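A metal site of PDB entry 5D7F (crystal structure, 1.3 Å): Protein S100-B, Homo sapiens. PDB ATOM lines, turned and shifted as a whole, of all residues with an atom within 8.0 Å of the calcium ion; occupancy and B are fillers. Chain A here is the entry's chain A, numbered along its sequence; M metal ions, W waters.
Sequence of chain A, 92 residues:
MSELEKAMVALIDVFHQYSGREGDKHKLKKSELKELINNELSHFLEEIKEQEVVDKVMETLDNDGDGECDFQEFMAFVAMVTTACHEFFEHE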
ATOM      1  N   LYS A  27      25.148   1.437  16.816  1.00  0.00           N
ATOM      2  CA  LYS A  27      26.264   0.745  16.228  1.00  0.00           C
ATOM      3  C   LYS A  27      27.572   1.431  16.623  1.00  0.00           C
ATOM      4  O   LYS A  27      27.585   2.683  16.901  1.00  0.00           O
ATOM      5  CB  LYS A  27      26.157   0.751  14.710  1.00  0.00           C
ATOM      6  CG  LYS A  27      24.894   0.070  14.168  1.00  0.00           C
ATOM      7  CD  LYS A  27      24.874   0.118  12.645  1.00  0.00           C
ATOM      8  CE  LYS A  27      23.584  -0.486  12.034  1.00  0.00           C
ATOM      9  NZ  LYS A  27      23.599  -0.344  10.514  1.00  0.00           N
ATOM     10  N   LEU A  28      28.624   0.616  16.627  1.00  0.00           N
ATOM     11  CA  LEU A  28      30.010   1.050  16.817  1.00  0.00           C
ATOM     12  C   LEU A  28      30.659   1.362  15.487  1.00  0.00           C
ATOM     13  O   LEU A  28      30.858   0.476  14.657  1.00  0.00           O
ATOM     14  CB  LEU A  28      30.823  -0.051  17.530  1.00  0.00           C
ATOM     15  CG  LEU A  28      30.318  -0.505  18.884  1.00  0.00           C
ATOM     16  CD1 LEU A  28      30.987  -1.855  19.268  1.00  0.00           C
ATOM     17  CD2 LEU A  28      30.618   0.519  19.966  1.00  0.00           C
ATOM     18  N   MET A  58      37.560  -4.218  12.429  1.00  0.00           N
ATOM     19  CA  MET A  58      36.220  -3.926  11.937  1.00  0.00           C
ATOM     20  C   MET A  58      35.837  -4.834  10.757  1.00  0.00           C
ATOM     21  O   MET A  58      34.738  -5.339  10.698  1.00  0.00           O
ATOM     22  CB  MET A  58      36.073  -2.450  11.537  1.00  0.00           C
ATOM     23  CG  MET A  58      34.672  -2.089  11.016  1.00  0.00           C
ATOM     24  SD  MET A  58      33.388  -2.256  12.252  1.00  0.00           S
ATOM     25  CE  MET A  58      33.625  -0.727  13.151  1.00  0.00           C
ATOM     26  N   LEU A  61      34.719  -8.219  12.112  1.00  0.00           N
ATOM     27  CA  LEU A  61      33.500  -8.196  12.902  1.00  0.00           C
ATOM     28  C   LEU A  61      32.254  -7.787  12.128  1.00  0.00           C
ATOM     29  O   LEU A  61      31.126  -8.150  12.471  1.00  0.00           O
ATOM     30  CB  LEU A  61      33.657  -7.298  14.114  1.00  0.00           C
ATOM     31  CG  LEU A  61      34.707  -7.688  15.142  1.00  0.00           C
ATOM     32  CD1 LEU A  61      34.556  -6.738  16.319  1.00  0.00           C
ATOM     33  CD2 LEU A  61      34.534  -9.181  15.535  1.00  0.00           C
ATOM     34  N   ASP A  62      32.453  -7.032  11.053  1.00  0.00           N
ATOM     35  CA  ASP A  62      31.346  -6.440  10.290  1.00  0.00           C
ATOM     36  C   ASP A  62      30.792  -7.423   9.256  1.00  0.00           C
ATOM     37  O   ASP A  62      31.122  -7.369   8.043  1.00  0.00           O
ATOM     38  CB  ASP A  62      31.836  -5.165   9.563  1.00  0.00           C
ATOM     39  CG  ASP A  62      30.751  -4.546   8.754  1.00  0.00           C
ATOM     40  OD1 ASP A  62      29.557  -4.761   9.039  1.00  0.00           O
ATOM     41  OD2 ASP A  62      31.093  -3.865   7.787  1.00  0.00           O
ATOM     42  N   ASN A  63      29.938  -8.329   9.706  1.00  0.00           N
ATOM     43  CA  ASN A  63      29.459  -9.388   8.842  1.00  0.00           C
ATOM     44  C   ASN A  63      28.466  -8.931   7.792  1.00  0.00           C
ATOM     45  O   ASN A  63      28.301  -9.598   6.784  1.00  0.00           O
ATOM     46  CB  ASN A  63      28.835 -10.495   9.705  1.00  0.00           C
ATOM     47  CG  ASN A  63      29.869 -11.218  10.581  1.00  0.00           C
ATOM     48  OD1 ASN A  63      31.014 -11.422  10.160  1.00  0.00           O
ATOM     49  ND2 ASN A  63      29.465 -11.559  11.794  1.00  0.00           N
ATOM     50  N   ASP A  64      27.783  -7.811   8.014  1.00  0.00           N
ATOM     51  CA  ASP A  64      26.826  -7.325   7.024  1.00  0.00           C
ATOM     52  C   ASP A  64      27.328  -6.195   6.114  1.00  0.00           C
ATOM     53  O   ASP A  64      26.524  -5.676   5.308  1.00  0.00           O
ATOM     54  CB  ASP A  64      25.465  -6.992   7.650  1.00  0.00           C
ATOM     55  CG  ASP A  64      25.490  -5.774   8.575  1.00  0.00           C
ATOM     56  OD1 ASP A  64      26.529  -5.139   8.742  1.00  0.00           O
ATOM     57  OD2 ASP A  64      24.421  -5.473   9.176  1.00  0.00           O
ATOM     58  N   GLY A  65      28.602  -5.800   6.225  1.00  0.00           N
ATOM     59  CA  GLY A  65      29.274  -4.911   5.299  1.00  0.00           C
ATOM     60  C   GLY A  65      28.927  -3.439   5.378  1.00  0.00           C
ATOM     61  O   GLY A  65      29.284  -2.723   4.481  1.00  0.00           O
ATOM     62  N   ASP A  66      28.248  -2.987   6.433  1.00  0.00           N
ATOM     63  CA  ASP A  66      27.903  -1.573   6.587  1.00  0.00           C
ATOM     64  C   ASP A  66      28.975  -0.675   7.200  1.00  0.00           C
ATOM     65  O   ASP A  66      28.742   0.546   7.382  1.00  0.00           O
ATOM     66  CB  ASP A  66      26.568  -1.406   7.315  1.00  0.00           C
ATOM     67  CG  ASP A  66      26.648  -1.721   8.802  1.00  0.00           C
ATOM     68  OD1 ASP A  66      27.656  -2.317   9.267  1.00  0.00           O
ATOM     69  OD2 ASP A  66      25.657  -1.411   9.509  1.00  0.00           O
ATOM     70  N   GLY A  67      30.123  -1.263   7.527  1.00  0.00           N
ATOM     71  CA  GLY A  67      31.272  -0.543   8.037  1.00  0.00           C
ATOM     72  C   GLY A  67      31.162  -0.258   9.525  1.00  0.00           C
ATOM     73  O   GLY A  67      32.003   0.456  10.097  1.00  0.00           O
ATOM     74  N   GLU A  68      30.132  -0.783  10.197  1.00  0.00           N
ATOM     75  CA  GLU A  68      29.978  -0.596  11.631  1.00  0.00           C
ATOM     76  C   GLU A  68      29.715  -1.937  12.300  1.00  0.00           C
ATOM     77  O   GLU A  68      29.338  -2.950  11.632  1.00  0.00           O
ATOM     78  CB  GLU A  68      28.832   0.343  11.979  1.00  0.00           C
ATOM     79  CG  GLU A  68      29.013   1.741  11.309  1.00  0.00           C
ATOM     80  CD  GLU A  68      28.427   2.893  12.109  1.00  0.00           C
ATOM     81  OE1 GLU A  68      28.342   2.796  13.341  1.00  0.00           O
ATOM     82  OE2 GLU A  68      28.041   3.904  11.528  1.00  0.00           O
ATOM     83  N   CYS A  69      29.890  -1.964  13.623  1.00  0.00           N
ATOM     84  CA  CYS A  69      29.642  -3.165  14.420  1.00  0.00           C
ATOM     85  C   CYS A  69      28.363  -2.989  15.224  1.00  0.00           C
ATOM     86  O   CYS A  69      28.285  -2.160  16.137  1.00  0.00           O
ATOM     87  CB  CYS A  69      30.857  -3.431  15.316  1.00  0.00           C
ATOM     88  SG  CYS A  69      30.697  -4.903  16.334  1.00  0.00           S
ATOM     89  N   ASP A  70      27.322  -3.721  14.846  1.00  0.00           N
ATOM     90  CA  ASP A  70      26.056  -3.648  15.590  1.00  0.00           C
ATOM     91  C   ASP A  70      26.103  -4.548  16.829  1.00  0.00           C
ATOM     92  O   ASP A  70      27.123  -5.171  17.141  1.00  0.00           O
ATOM     93  CB  ASP A  70      24.812  -3.894  14.697  1.00  0.00           C
ATOM     94  CG  ASP A  70      24.721  -5.312  14.169  1.00  0.00           C
ATOM     95  OD1 ASP A  70      25.406  -6.227  14.644  1.00  0.00           O
ATOM     96  OD2 ASP A  70      23.910  -5.535  13.267  1.00  0.00           O
ATOM     97  N   PHE A  71      24.966  -4.672  17.534  1.00  0.00           N
ATOM     98  CA  PHE A  71      24.977  -5.440  18.781  1.00  0.00           C
ATOM     99  C   PHE A  71      25.212  -6.926  18.561  1.00  0.00           C
ATOM    100  O   PHE A  71      25.974  -7.542  19.290  1.00  0.00           O
ATOM    101  CB  PHE A  71      23.731  -5.184  19.637  1.00  0.00           C
ATOM    102  CG  PHE A  71      23.818  -5.815  20.984  1.00  0.00           C
ATOM    103  CD1 PHE A  71      24.667  -5.315  21.949  1.00  0.00           C
ATOM    104  CD2 PHE A  71      23.110  -7.009  21.255  1.00  0.00           C
ATOM    105  CE1 PHE A  71      24.797  -5.934  23.189  1.00  0.00           C
ATOM    106  CE2 PHE A  71      23.219  -7.621  22.507  1.00  0.00           C
ATOM    107  CZ  PHE A  71      24.054  -7.090  23.461  1.00  0.00           C
ATOM    108  N   GLU A  73      26.864  -8.264  16.061  1.00  0.00           N
ATOM    109  CA  GLU A  73      28.271  -8.387  15.674  1.00  0.00           C
ATOM    110  C   GLU A  73      29.175  -8.225  16.888  1.00  0.00           C
ATOM    111  O   GLU A  73      30.194  -8.922  17.013  1.00  0.00           O
ATOM    112  CB  GLU A  73      28.594  -7.371  14.560  1.00  0.00           C
ATOM    113  CG  GLU A  73      27.954  -7.758  13.225  1.00  0.00           C
ATOM    114  CD  GLU A  73      27.879  -6.611  12.252  1.00  0.00           C
ATOM    115  OE1 GLU A  73      28.038  -5.427  12.656  1.00  0.00           O
ATOM    116  OE2 GLU A  73      27.714  -6.830  11.032  1.00  0.00           O
ATOM    117  N   PHE A  74      28.813  -7.320  17.796  1.00  0.00           N
ATOM    118  CA  PHE A  74      29.556  -7.158  19.052  1.00  0.00           C
ATOM    119  C   PHE A  74      29.458  -8.449  19.908  1.00  0.00           C
ATOM    120  O   PHE A  74      30.450  -8.900  20.492  1.00  0.00           O
ATOM    121  CB  PHE A  74      29.003  -5.979  19.817  1.00  0.00           C
ATOM    122  CG  PHE A  74      29.567  -5.836  21.188  1.00  0.00           C
ATOM    123  CD1 PHE A  74      30.899  -5.438  21.334  1.00  0.00           C
ATOM    124  CD2 PHE A  74      28.815  -6.137  22.333  1.00  0.00           C
ATOM    125  CE1 PHE A  74      31.470  -5.285  22.593  1.00  0.00           C
ATOM    126  CE2 PHE A  74      29.384  -5.945  23.620  1.00  0.00           C
ATOM    127  CZ  PHE A  74      30.730  -5.551  23.723  1.00  0.00           C
HETATM  128 CA    CA M   1      27.847  -4.284  10.494  1.00  0.00          CA
HETATM  129  O   HOH W   1      25.753  -3.501  11.396  1.00  0.00           O
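The calcium ion is bound by OD1 of Asp 62 (2.3 Å), O of Glu 68 (2.3 Å), OD1 of Asp 66 (2.3 Å), OD1 of Asp 64 (2.4 Å), water W1 (2.4 Å), OE1 of Glu 73 (2.5 Å) and OE2 of Glu 73 (2.6 Å).
The calcium ion has seven donor atoms within binding distance.
The backbone NH (N) of Gly 65 lies close to the side-chain carboxylate (OD1) of Asp 62.
The backbone NH (N) of Gly 67 sits at hydrogen-bond distance from the side-chain carboxylate (OD2) of Asp 62, at 2.8 Å.
The side-chain carboxylate (OD2) of Asp 66 is in salt-bridge range of the side-chain amino group (NZ) of Lys 27 (2.5 Å).
The side-chain carboxylate (OD1) of Asp 70 sits at hydrogen-bond distance from the backbone NH (N) of Glu 73.
The side-chain carboxylate (OE2) of Glu 73 sits close to the backbone NH (N) of Asn 63, 3.0 Å away.
Five residues have an atom within 4 Å of the calcium ion: Asp 62, Asp 64, Asp 66, Glu 68 and Glu 73.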
